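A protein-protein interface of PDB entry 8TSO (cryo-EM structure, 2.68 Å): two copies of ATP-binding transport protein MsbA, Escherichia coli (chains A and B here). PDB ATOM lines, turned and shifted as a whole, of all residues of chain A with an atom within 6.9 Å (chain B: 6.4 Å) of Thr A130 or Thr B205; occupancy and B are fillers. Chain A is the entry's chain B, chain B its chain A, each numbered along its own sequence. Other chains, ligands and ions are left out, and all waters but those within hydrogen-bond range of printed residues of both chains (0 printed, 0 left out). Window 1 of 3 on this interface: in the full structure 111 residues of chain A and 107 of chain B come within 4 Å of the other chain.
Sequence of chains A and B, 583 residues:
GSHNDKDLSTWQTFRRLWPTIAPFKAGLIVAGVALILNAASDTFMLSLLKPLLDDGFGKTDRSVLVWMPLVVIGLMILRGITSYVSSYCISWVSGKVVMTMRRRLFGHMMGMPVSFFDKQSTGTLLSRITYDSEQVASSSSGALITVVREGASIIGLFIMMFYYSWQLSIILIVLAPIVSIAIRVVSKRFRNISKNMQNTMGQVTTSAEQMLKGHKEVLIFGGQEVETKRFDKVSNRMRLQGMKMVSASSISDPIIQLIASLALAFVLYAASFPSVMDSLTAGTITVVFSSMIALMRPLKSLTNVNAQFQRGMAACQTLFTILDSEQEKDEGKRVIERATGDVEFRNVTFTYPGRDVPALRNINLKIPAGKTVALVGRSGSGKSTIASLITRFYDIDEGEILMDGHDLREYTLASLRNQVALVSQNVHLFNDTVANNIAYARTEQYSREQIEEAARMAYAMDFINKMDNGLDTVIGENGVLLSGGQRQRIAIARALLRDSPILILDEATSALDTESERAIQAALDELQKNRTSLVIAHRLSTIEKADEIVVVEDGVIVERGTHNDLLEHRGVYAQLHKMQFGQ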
ATOM      1  N   VAL A  98      -6.341 -38.308  15.054  1.00  0.00           N
ATOM      2  CA  VAL A  98      -6.263 -36.903  15.456  1.00  0.00           C
ATOM      3  C   VAL A  98      -7.488 -36.509  16.274  1.00  0.00           C
ATOM      4  O   VAL A  98      -7.376 -35.807  17.287  1.00  0.00           O
ATOM      5  CB  VAL A  98      -6.088 -36.002  14.220  1.00  0.00           C
ATOM      6  CG1 VAL A  98      -6.369 -34.553  14.568  1.00  0.00           C
ATOM      7  CG2 VAL A  98      -4.689 -36.142  13.683  1.00  0.00           C
ATOM      8  N   ARG A 102      -7.580 -35.226  20.142  1.00  0.00           N
ATOM      9  CA  ARG A 102      -8.228 -33.970  20.506  1.00  0.00           C
ATOM     10  C   ARG A 102      -9.237 -34.180  21.625  1.00  0.00           C
ATOM     11  O   ARG A 102      -9.283 -33.411  22.593  1.00  0.00           O
ATOM     12  CB  ARG A 102      -8.912 -33.360  19.284  1.00  0.00           C
ATOM     13  CG  ARG A 102      -7.988 -32.621  18.352  1.00  0.00           C
ATOM     14  CD  ARG A 102      -8.748 -31.611  17.520  1.00  0.00           C
ATOM     15  NE  ARG A 102      -7.855 -30.822  16.684  1.00  0.00           N
ATOM     16  CZ  ARG A 102      -7.727 -30.973  15.374  1.00  0.00           C
ATOM     17  NH1 ARG A 102      -8.436 -31.869  14.709  1.00  0.00           N
ATOM     18  NH2 ARG A 102      -6.867 -30.206  14.713  1.00  0.00           N
ATOM     19  N   LEU A 105      -7.399 -34.905  24.962  1.00  0.00           N
ATOM     20  CA  LEU A 105      -6.864 -33.674  25.533  1.00  0.00           C
ATOM     21  C   LEU A 105      -7.969 -32.817  26.133  1.00  0.00           C
ATOM     22  O   LEU A 105      -7.804 -32.252  27.220  1.00  0.00           O
ATOM     23  CB  LEU A 105      -6.105 -32.882  24.471  1.00  0.00           C
ATOM     24  CG  LEU A 105      -4.623 -33.184  24.287  1.00  0.00           C
ATOM     25  CD1 LEU A 105      -4.081 -32.380  23.126  1.00  0.00           C
ATOM     26  CD2 LEU A 105      -3.860 -32.876  25.559  1.00  0.00           C
ATOM     27  N   GLY A 123      -4.042 -19.608  25.689  1.00  0.00           N
ATOM     28  CA  GLY A 123      -3.512 -19.846  24.357  1.00  0.00           C
ATOM     29  C   GLY A 123      -2.674 -21.107  24.270  1.00  0.00           C
ATOM     30  O   GLY A 123      -2.661 -21.784  23.241  1.00  0.00           O
ATOM     31  N   LEU A 125      -3.121 -23.977  25.997  1.00  0.00           N
ATOM     32  CA  LEU A 125      -4.041 -25.106  25.902  1.00  0.00           C
ATOM     33  C   LEU A 125      -4.750 -25.128  24.553  1.00  0.00           C
ATOM     34  O   LEU A 125      -4.966 -26.198  23.969  1.00  0.00           O
ATOM     35  CB  LEU A 125      -5.055 -25.036  27.042  1.00  0.00           C
ATOM     36  CG  LEU A 125      -4.485 -24.734  28.430  1.00  0.00           C
ATOM     37  CD1 LEU A 125      -5.594 -24.684  29.460  1.00  0.00           C
ATOM     38  CD2 LEU A 125      -3.438 -25.759  28.820  1.00  0.00           C
ATOM     39  N   LEU A 126      -5.122 -23.951  24.046  1.00  0.00           N
ATOM     40  CA  LEU A 126      -5.765 -23.877  22.740  1.00  0.00           C
ATOM     41  C   LEU A 126      -4.852 -24.410  21.645  1.00  0.00           C
ATOM     42  O   LEU A 126      -5.299 -25.149  20.763  1.00  0.00           O
ATOM     43  CB  LEU A 126      -6.167 -22.437  22.438  1.00  0.00           C
ATOM     44  CG  LEU A 126      -7.295 -21.843  23.277  1.00  0.00           C
ATOM     45  CD1 LEU A 126      -7.598 -20.448  22.790  1.00  0.00           C
ATOM     46  CD2 LEU A 126      -8.527 -22.715  23.215  1.00  0.00           C
ATOM     47  N   SER A 127      -3.572 -24.041  21.683  1.00  0.00           N
ATOM     48  CA  SER A 127      -2.628 -24.548  20.695  1.00  0.00           C
ATOM     49  C   SER A 127      -2.387 -26.039  20.862  1.00  0.00           C
ATOM     50  O   SER A 127      -2.183 -26.743  19.869  1.00  0.00           O
ATOM     51  CB  SER A 127      -1.311 -23.784  20.786  1.00  0.00           C
ATOM     52  OG  SER A 127      -1.496 -22.431  20.419  1.00  0.00           O
ATOM     53  N   ARG A 128      -2.388 -26.536  22.099  1.00  0.00           N
ATOM     54  CA  ARG A 128      -2.258 -27.974  22.302  1.00  0.00           C
ATOM     55  C   ARG A 128      -3.412 -28.724  21.653  1.00  0.00           C
ATOM     56  O   ARG A 128      -3.208 -29.763  21.017  1.00  0.00           O
ATOM     57  CB  ARG A 128      -2.186 -28.294  23.792  1.00  0.00           C
ATOM     58  CG  ARG A 128      -0.901 -27.857  24.455  1.00  0.00           C
ATOM     59  CD  ARG A 128      -1.017 -27.960  25.958  1.00  0.00           C
ATOM     60  NE  ARG A 128       0.197 -27.524  26.635  1.00  0.00           N
ATOM     61  CZ  ARG A 128       0.346 -27.494  27.952  1.00  0.00           C
ATOM     62  NH1 ARG A 128      -0.625 -27.878  28.765  1.00  0.00           N
ATOM     63  NH2 ARG A 128       1.497 -27.072  28.465  1.00  0.00           N
ATOM     64  N   ILE A 129      -4.634 -28.211  21.803  1.00  0.00           N
ATOM     65  CA  ILE A 129      -5.791 -28.884  21.213  1.00  0.00           C
ATOM     66  C   ILE A 129      -5.778 -28.754  19.693  1.00  0.00           C
ATOM     67  O   ILE A 129      -6.022 -29.728  18.972  1.00  0.00           O
ATOM     68  CB  ILE A 129      -7.099 -28.343  21.816  1.00  0.00           C
ATOM     69  CG1 ILE A 129      -7.338 -28.956  23.195  1.00  0.00           C
ATOM     70  CG2 ILE A 129      -8.272 -28.637  20.898  1.00  0.00           C
ATOM     71  CD1 ILE A 129      -8.738 -28.750  23.719  1.00  0.00           C
ATOM     72  N   THR A 130      -5.485 -27.559  19.183  1.00  0.00           N
ATOM     73  CA  THR A 130      -5.677 -27.304  17.758  1.00  0.00           C
ATOM     74  C   THR A 130      -4.443 -27.652  16.933  1.00  0.00           C
ATOM     75  O   THR A 130      -4.570 -28.210  15.839  1.00  0.00           O
ATOM     76  CB  THR A 130      -6.064 -25.842  17.532  1.00  0.00           C
ATOM     77  OG1 THR A 130      -5.077 -24.985  18.112  1.00  0.00           O
ATOM     78  CG2 THR A 130      -7.413 -25.546  18.161  1.00  0.00           C
ATOM     79  N   TYR A 131      -3.250 -27.334  17.427  1.00  0.00           N
ATOM     80  CA  TYR A 131      -2.028 -27.512  16.652  1.00  0.00           C
ATOM     81  C   TYR A 131      -1.287 -28.797  16.984  1.00  0.00           C
ATOM     82  O   TYR A 131      -0.937 -29.554  16.074  1.00  0.00           O
ATOM     83  CB  TYR A 131      -1.097 -26.307  16.855  1.00  0.00           C
ATOM     84  CG  TYR A 131       0.224 -26.418  16.127  1.00  0.00           C
ATOM     85  CD1 TYR A 131       0.320 -26.116  14.778  1.00  0.00           C
ATOM     86  CD2 TYR A 131       1.376 -26.817  16.792  1.00  0.00           C
ATOM     87  CE1 TYR A 131       1.522 -26.213  14.111  1.00  0.00           C
ATOM     88  CE2 TYR A 131       2.581 -26.919  16.133  1.00  0.00           C
ATOM     89  CZ  TYR A 131       2.648 -26.615  14.793  1.00  0.00           C
ATOM     90  OH  TYR A 131       3.847 -26.712  14.128  1.00  0.00           O
ATOM     91  N   ASP A 132      -1.034 -29.067  18.267  1.00  0.00           N
ATOM     92  CA  ASP A 132      -0.200 -30.208  18.634  1.00  0.00           C
ATOM     93  C   ASP A 132      -0.871 -31.531  18.291  1.00  0.00           C
ATOM     94  O   ASP A 132      -0.192 -32.509  17.966  1.00  0.00           O
ATOM     95  CB  ASP A 132       0.142 -30.158  20.122  1.00  0.00           C
ATOM     96  CG  ASP A 132       0.849 -28.880  20.517  1.00  0.00           C
ATOM     97  OD1 ASP A 132       0.906 -27.949  19.691  1.00  0.00           O
ATOM     98  OD2 ASP A 132       1.356 -28.810  21.655  1.00  0.00           O
ATOM     99  N   SER A 133      -2.201 -31.587  18.375  1.00  0.00           N
ATOM    100  CA  SER A 133      -2.907 -32.828  18.071  1.00  0.00           C
ATOM    101  C   SER A 133      -2.839 -33.156  16.584  1.00  0.00           C
ATOM    102  O   SER A 133      -2.786 -34.331  16.206  1.00  0.00           O
ATOM    103  CB  SER A 133      -4.358 -32.731  18.533  1.00  0.00           C
ATOM    104  OG  SER A 133      -4.427 -32.397  19.905  1.00  0.00           O
ATOM    105  N   GLU A 134      -2.846 -32.131  15.729  1.00  0.00           N
ATOM    106  CA  GLU A 134      -2.817 -32.363  14.290  1.00  0.00           C
ATOM    107  C   GLU A 134      -1.491 -32.963  13.838  1.00  0.00           C
ATOM    108  O   GLU A 134      -1.456 -33.720  12.863  1.00  0.00           O
ATOM    109  CB  GLU A 134      -3.096 -31.054  13.550  1.00  0.00           C
ATOM    110  CG  GLU A 134      -3.041 -31.146  12.032  1.00  0.00           C
ATOM    111  CD  GLU A 134      -4.104 -32.059  11.451  1.00  0.00           C
ATOM    112  OE1 GLU A 134      -5.186 -32.183  12.059  1.00  0.00           O
ATOM    113  OE2 GLU A 134      -3.861 -32.646  10.377  1.00  0.00           O
ATOM    114  N   GLN A 135      -0.396 -32.648  14.531  1.00  0.00           N
ATOM    115  CA  GLN A 135       0.920 -33.133  14.126  1.00  0.00           C
ATOM    116  C   GLN A 135       1.064 -34.640  14.267  1.00  0.00           C
ATOM    117  O   GLN A 135       1.976 -35.213  13.663  1.00  0.00           O
ATOM    118  CB  GLN A 135       2.011 -32.430  14.933  1.00  0.00           C
ATOM    119  CG  GLN A 135       1.792 -30.939  15.089  1.00  0.00           C
ATOM    120  CD  GLN A 135       1.559 -30.246  13.765  1.00  0.00           C
ATOM    121  OE1 GLN A 135       2.307 -30.441  12.811  1.00  0.00           O
ATOM    122  NE2 GLN A 135       0.506 -29.442  13.696  1.00  0.00           N
ATOM    123  N   THR A 205      -0.437 -17.799  19.830  1.00  0.00           N
ATOM    124  CA  THR A 205      -1.877 -17.779  20.213  1.00  0.00           C
ATOM    125  C   THR A 205      -2.103 -16.899  21.447  1.00  0.00           C
ATOM    126  O   THR A 205      -3.115 -16.192  21.473  1.00  0.00           O
ATOM    127  CB  THR A 205      -2.389 -19.204  20.439  1.00  0.00           C
ATOM    128  OG1 THR A 205      -1.905 -20.014  19.367  1.00  0.00           O
ATOM    129  CG2 THR A 205      -3.896 -19.289  20.519  1.00  0.00           C
ATOM    130  N   GLU A 209      -4.270 -13.324  21.743  1.00  0.00           N
ATOM    131  CA  GLU A 209      -5.338 -13.372  22.772  1.00  0.00           C
ATOM    132  C   GLU A 209      -5.159 -12.256  23.800  1.00  0.00           C
ATOM    133  O   GLU A 209      -6.177 -11.744  24.278  1.00  0.00           O
ATOM    134  CB  GLU A 209      -5.249 -14.715  23.486  1.00  0.00           C
ATOM    135  CG  GLU A 209      -6.560 -15.465  23.555  1.00  0.00           C
ATOM    136  CD  GLU A 209      -6.435 -16.798  24.269  1.00  0.00           C
ATOM    137  OE1 GLU A 209      -5.321 -17.112  24.728  1.00  0.00           O
ATOM    138  OE2 GLU A 209      -7.448 -17.515  24.363  1.00  0.00           O
ATOM    139  N   SER B 121     -16.274 -13.808  18.065  1.00  0.00           N
ATOM    140  CA  SER B 121     -15.723 -14.718  19.053  1.00  0.00           C
ATOM    141  C   SER B 121     -14.203 -14.688  18.973  1.00  0.00           C
ATOM    142  O   SER B 121     -13.632 -14.563  17.887  1.00  0.00           O
ATOM    143  CB  SER B 121     -16.233 -16.142  18.833  1.00  0.00           C
ATOM    144  OG  SER B 121     -15.420 -17.080  19.509  1.00  0.00           O
ATOM    145  N   THR B 122     -13.554 -14.790  20.134  1.00  0.00           N
ATOM    146  CA  THR B 122     -12.096 -14.765  20.171  1.00  0.00           C
ATOM    147  C   THR B 122     -11.495 -15.946  19.421  1.00  0.00           C
ATOM    148  O   THR B 122     -10.479 -15.791  18.733  1.00  0.00           O
ATOM    149  CB  THR B 122     -11.614 -14.753  21.623  1.00  0.00           C
ATOM    150  OG1 THR B 122     -12.259 -13.688  22.328  1.00  0.00           O
ATOM    151  CG2 THR B 122     -10.113 -14.553  21.691  1.00  0.00           C
ATOM    152  N   GLY B 123     -12.109 -17.125  19.536  1.00  0.00           N
ATOM    153  CA  GLY B 123     -11.574 -18.300  18.867  1.00  0.00           C
ATOM    154  C   GLY B 123     -11.534 -18.157  17.359  1.00  0.00           C
ATOM    155  O   GLY B 123     -10.623 -18.664  16.704  1.00  0.00           O
ATOM    156  N   THR B 124     -12.519 -17.462  16.789  1.00  0.00           N
ATOM    157  CA  THR B 124     -12.543 -17.249  15.344  1.00  0.00           C
ATOM    158  C   THR B 124     -11.330 -16.446  14.885  1.00  0.00           C
ATOM    159  O   THR B 124     -10.635 -16.829  13.936  1.00  0.00           O
ATOM    160  CB  THR B 124     -13.841 -16.545  14.953  1.00  0.00           C
ATOM    161  OG1 THR B 124     -14.948 -17.421  15.188  1.00  0.00           O
ATOM    162  CG2 THR B 124     -13.818 -16.150  13.488  1.00  0.00           C
ATOM    163  N   LEU B 126      -8.529 -16.009  16.566  1.00  0.00           N
ATOM    164  CA  LEU B 126      -7.331 -16.788  16.856  1.00  0.00           C
ATOM    165  C   LEU B 126      -7.060 -17.812  15.763  1.00  0.00           C
ATOM    166  O   LEU B 126      -5.912 -17.995  15.348  1.00  0.00           O
ATOM    167  CB  LEU B 126      -7.470 -17.482  18.207  1.00  0.00           C
ATOM    168  CG  LEU B 126      -7.414 -16.604  19.451  1.00  0.00           C
ATOM    169  CD1 LEU B 126      -7.321 -17.489  20.664  1.00  0.00           C
ATOM    170  CD2 LEU B 126      -6.238 -15.657  19.392  1.00  0.00           C
ATOM    171  N   SER B 127      -8.103 -18.497  15.293  1.00  0.00           N
ATOM    172  CA  SER B 127      -7.924 -19.458  14.214  1.00  0.00           C
ATOM    173  C   SER B 127      -7.550 -18.775  12.910  1.00  0.00           C
ATOM    174  O   SER B 127      -6.784 -19.334  12.119  1.00  0.00           O
ATOM    175  CB  SER B 127      -9.191 -20.289  14.033  1.00  0.00           C
ATOM    176  OG  SER B 127      -9.426 -21.089  15.175  1.00  0.00           O
ATOM    177  N   THR B 130      -3.797 -18.096  13.392  1.00  0.00           N
ATOM    178  CA  THR B 130      -2.909 -19.243  13.556  1.00  0.00           C
ATOM    179  C   THR B 130      -3.091 -20.282  12.456  1.00  0.00           C
ATOM    180  O   THR B 130      -2.111 -20.883  12.006  1.00  0.00           O
ATOM    181  CB  THR B 130      -3.124 -19.886  14.926  1.00  0.00           C
ATOM    182  OG1 THR B 130      -4.503 -20.234  15.085  1.00  0.00           O
ATOM    183  CG2 THR B 130      -2.722 -18.928  16.031  1.00  0.00           C
ATOM    184  N   THR B 200     -14.691 -24.622  10.562  1.00  0.00           N
ATOM    185  CA  THR B 200     -14.768 -25.639  11.608  1.00  0.00           C
ATOM    186  C   THR B 200     -13.575 -25.573  12.555  1.00  0.00           C
ATOM    187  O   THR B 200     -13.709 -25.895  13.738  1.00  0.00           O
ATOM    188  CB  THR B 200     -14.890 -27.031  10.991  1.00  0.00           C
ATOM    189  OG1 THR B 200     -13.784 -27.268  10.115  1.00  0.00           O
ATOM    190  CG2 THR B 200     -16.180 -27.150  10.208  1.00  0.00           C
ATOM    191  N   MET B 201     -12.405 -25.164  12.063  1.00  0.00           N
ATOM    192  CA  MET B 201     -11.266 -24.951  12.951  1.00  0.00           C
ATOM    193  C   MET B 201     -11.541 -23.809  13.921  1.00  0.00           C
ATOM    194  O   MET B 201     -11.231 -23.898  15.119  1.00  0.00           O
ATOM    195  CB  MET B 201     -10.008 -24.674  12.126  1.00  0.00           C
ATOM    196  CG  MET B 201      -8.703 -24.913  12.866  1.00  0.00           C
ATOM    197  SD  MET B 201      -8.191 -26.641  12.918  1.00  0.00           S
ATOM    198  CE  MET B 201      -8.814 -27.145  14.517  1.00  0.00           C
ATOM    199  N   GLY B 202     -12.128 -22.723  13.415  1.00  0.00           N
ATOM    200  CA  GLY B 202     -12.560 -21.657  14.306  1.00  0.00           C
ATOM    201  C   GLY B 202     -13.567 -22.139  15.332  1.00  0.00           C
ATOM    202  O   GLY B 202     -13.532 -21.737  16.497  1.00  0.00           O
ATOM    203  N   GLN B 203     -14.476 -23.022  14.908  1.00  0.00           N
ATOM    204  CA  GLN B 203     -15.464 -23.586  15.823  1.00  0.00           C
ATOM    205  C   GLN B 203     -14.806 -24.426  16.911  1.00  0.00           C
ATOM    206  O   GLN B 203     -15.218 -24.388  18.074  1.00  0.00           O
ATOM    207  CB  GLN B 203     -16.480 -24.427  15.051  1.00  0.00           C
ATOM    208  CG  GLN B 203     -17.326 -23.652  14.070  1.00  0.00           C
ATOM    209  CD  GLN B 203     -18.210 -24.556  13.242  1.00  0.00           C
ATOM    210  OE1 GLN B 203     -18.482 -25.693  13.624  1.00  0.00           O
ATOM    211  NE2 GLN B 203     -18.652 -24.063  12.092  1.00  0.00           N
ATOM    212  N   VAL B 204     -13.798 -25.220  16.542  1.00  0.00           N
ATOM    213  CA  VAL B 204     -13.078 -26.030  17.526  1.00  0.00           C
ATOM    214  C   VAL B 204     -12.407 -25.131  18.556  1.00  0.00           C
ATOM    215  O   VAL B 204     -12.482 -25.371  19.772  1.00  0.00           O
ATOM    216  CB  VAL B 204     -12.051 -26.940  16.827  1.00  0.00           C
ATOM    217  CG1 VAL B 204     -11.196 -27.662  17.850  1.00  0.00           C
ATOM    218  CG2 VAL B 204     -12.743 -27.945  15.930  1.00  0.00           C
ATOM    219  N   THR B 205     -11.744 -24.076  18.080  1.00  0.00           N
ATOM    220  CA  THR B 205     -11.083 -23.146  18.991  1.00  0.00           C
ATOM    221  C   THR B 205     -12.093 -22.482  19.921  1.00  0.00           C
ATOM    222  O   THR B 205     -11.853 -22.347  21.127  1.00  0.00           O
ATOM    223  CB  THR B 205     -10.309 -22.096  18.197  1.00  0.00           C
ATOM    224  OG1 THR B 205      -9.441 -22.748  17.265  1.00  0.00           O
ATOM    225  CG2 THR B 205      -9.473 -21.241  19.129  1.00  0.00           C
ATOM    226  N   THR B 206     -13.241 -22.075  19.375  1.00  0.00           N
ATOM    227  CA  THR B 206     -14.275 -21.439  20.185  1.00  0.00           C
ATOM    228  C   THR B 206     -14.841 -22.394  21.229  1.00  0.00           C
ATOM    229  O   THR B 206     -15.113 -21.997  22.364  1.00  0.00           O
ATOM    230  CB  THR B 206     -15.392 -20.914  19.284  1.00  0.00           C
ATOM    231  OG1 THR B 206     -14.831 -20.093  18.253  1.00  0.00           O
ATOM    232  CG2 THR B 206     -16.392 -20.107  20.087  1.00  0.00           C
ATOM    233  N   SER B 207     -15.050 -23.656  20.852  1.00  0.00           N
ATOM    234  CA  SER B 207     -15.582 -24.637  21.791  1.00  0.00           C
ATOM    235  C   SER B 207     -14.617 -24.867  22.948  1.00  0.00           C
ATOM    236  O   SER B 207     -15.023 -24.916  24.117  1.00  0.00           O
ATOM    237  CB  SER B 207     -15.877 -25.945  21.058  1.00  0.00           C
ATOM    238  OG  SER B 207     -16.551 -26.866  21.896  1.00  0.00           O
ATOM    239  N   ALA B 208     -13.326 -25.000  22.636  1.00  0.00           N
ATOM    240  CA  ALA B 208     -12.331 -25.153  23.693  1.00  0.00           C
ATOM    241  C   ALA B 208     -12.291 -23.919  24.590  1.00  0.00           C
ATOM    242  O   ALA B 208     -12.214 -24.033  25.821  1.00  0.00           O
ATOM    243  CB  ALA B 208     -10.958 -25.432  23.084  1.00  0.00           C
ATOM    244  N   GLU B 209     -12.357 -22.728  23.988  1.00  0.00           N
ATOM    245  CA  GLU B 209     -12.359 -21.491  24.762  1.00  0.00           C
ATOM    246  C   GLU B 209     -13.556 -21.416  25.698  1.00  0.00           C
ATOM    247  O   GLU B 209     -13.437 -20.980  26.845  1.00  0.00           O
ATOM    248  CB  GLU B 209     -12.370 -20.285  23.829  1.00  0.00           C
ATOM    249  CG  GLU B 209     -11.054 -19.969  23.186  1.00  0.00           C
ATOM    250  CD  GLU B 209     -11.106 -18.667  22.424  1.00  0.00           C
ATOM    251  OE1 GLU B 209     -12.226 -18.180  22.164  1.00  0.00           O
ATOM    252  OE2 GLU B 209     -10.034 -18.127  22.095  1.00  0.00           O
ATOM    253  N   GLN B 210     -14.731 -21.804  25.204  1.00  0.00           N
ATOM    254  CA  GLN B 210     -15.936 -21.720  26.019  1.00  0.00           C
ATOM    255  C   GLN B 210     -15.908 -22.735  27.150  1.00  0.00           C
ATOM    256  O   GLN B 210     -16.414 -22.465  28.246  1.00  0.00           O
ATOM    257  CB  GLN B 210     -17.175 -21.907  25.146  1.00  0.00           C
ATOM    258  CG  GLN B 210     -17.452 -20.724  24.239  1.00  0.00           C
ATOM    259  CD  GLN B 210     -17.565 -19.420  25.003  1.00  0.00           C
ATOM    260  OE1 GLN B 210     -18.147 -19.369  26.085  1.00  0.00           O
ATOM    261  NE2 GLN B 210     -16.992 -18.359  24.450  1.00  0.00           N
ATOM    262  N   PHE B 231     -18.172 -31.172  22.406  1.00  0.00           N
ATOM    263  CA  PHE B 231     -16.883 -31.130  21.725  1.00  0.00           C
ATOM    264  C   PHE B 231     -16.699 -32.301  20.768  1.00  0.00           C
ATOM    265  O   PHE B 231     -15.981 -32.170  19.769  1.00  0.00           O
ATOM    266  CB  PHE B 231     -15.744 -31.106  22.741  1.00  0.00           C
ATOM    267  CG  PHE B 231     -14.391 -30.914  22.123  1.00  0.00           C
ATOM    268  CD1 PHE B 231     -14.012 -29.681  21.622  1.00  0.00           C
ATOM    269  CD2 PHE B 231     -13.499 -31.967  22.039  1.00  0.00           C
ATOM    270  CE1 PHE B 231     -12.772 -29.504  21.053  1.00  0.00           C
ATOM    271  CE2 PHE B 231     -12.260 -31.792  21.471  1.00  0.00           C
ATOM    272  CZ  PHE B 231     -11.897 -30.562  20.976  1.00  0.00           C
ATOM    273  N   VAL B 234     -17.988 -31.209  17.331  1.00  0.00           N
ATOM    274  CA  VAL B 234     -17.122 -30.314  16.567  1.00  0.00           C
ATOM    275  C   VAL B 234     -15.871 -31.043  16.088  1.00  0.00           C
ATOM    276  O   VAL B 234     -15.395 -30.821  14.964  1.00  0.00           O
ATOM    277  CB  VAL B 234     -16.769 -29.072  17.406  1.00  0.00           C
ATOM    278  CG1 VAL B 234     -16.304 -27.945  16.508  1.00  0.00           C
ATOM    279  CG2 VAL B 234     -17.966 -28.633  18.223  1.00  0.00           C
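The side-chain carboxylate (OE2) of Glu B209 sits close to the side-chain carboxylate (OE2) of Glu A209.
The backbone NH of Gly B123 is in hydrogen-bond range of the side-chain carboxylate of Glu B209, at 2.8 Å.
The backbone carbonyl oxygen (O) of Leu B126 is in hydrogen-bond range of the side-chain hydroxyl (OG1) of Thr B130.
O of Thr A130 is in hydrogen-bond range of NH2 of Arg A102, 3.2 Å away.
NH2 of Arg A102 is in salt-bridge range of OE1 of Glu A134.
N of Gly A123 is in hydrogen-bond range of OE1 of Glu A209, 3.0 Å away.
The side-chain hydroxyl (OG1) of Thr A130 lies within hydrogen-bond range of the backbone carbonyl oxygen (O) of Leu A126 (2.7 Å).
Among the printed residues, merely in contact across the chains: Arg A102 with Met B201, Arg A102 with Phe B231, Leu A126 with Leu B126, Leu A126 with Thr B205, Leu A126 with Ala B208, Leu A126 with Glu B209, Thr A130 with Thr B205, Thr A205 with Leu B126, Thr A205 with Thr B130 and Glu A209 with Leu B126.
Of chain B, only Thr B205 (3.6 Å) comes within 4 Å of Thr A130.
Of chain A, only Leu A126 (3.9 Å) and Thr A130 (3.6 Å) come within 4 Å of Thr B205.
Printed residues of chain A within 4 Å of Phe B231: Arg A102.
Of the printed residues of chain A, Ala B208 touches Leu A126 (3.6 Å).
Val A98 touches none of the printed residues of chain B.
The nearest residue of chain B that does not touch Thr A130 is Met B201 (4.2 Å).
The nearest printed residue of chain A that does not touch Glu B209 is Thr A205 (6.4 Å).
Printed residues of chain A that touch a printed residue of chain B: Arg A102, Leu A126, Thr A130, Thr A205 and Glu A209.
Of the 20 printed residues of chain B, 7 touch a printed residue of chain A.
Hydrophobic or aromatic side chains of chain B that line the printed part of chain A: Leu B126, Met B201, Ala B208 and Phe B231.
Along chain B the printed residues that touch a printed residue of chain A span positions 126 to 231.
Among the printed residues, no Asp or Glu carboxylate lies within 4 Å of a Lys or Arg side-chain nitrogen of the other chain.
Leu B126 touches its own counterpart, Leu A126.
Leu A126 touches Thr B205, and with the chains exchanged Thr A205 touches Leu B126.
Leu A126 touches Glu B209, and with the chains exchanged Glu A209 touches Leu B126.
Glu B209 touches its own counterpart, Glu A209.
Of the 11 pairs that touch across the chains among the printed residues, 8 have their exchanged pair printed and touching as well.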
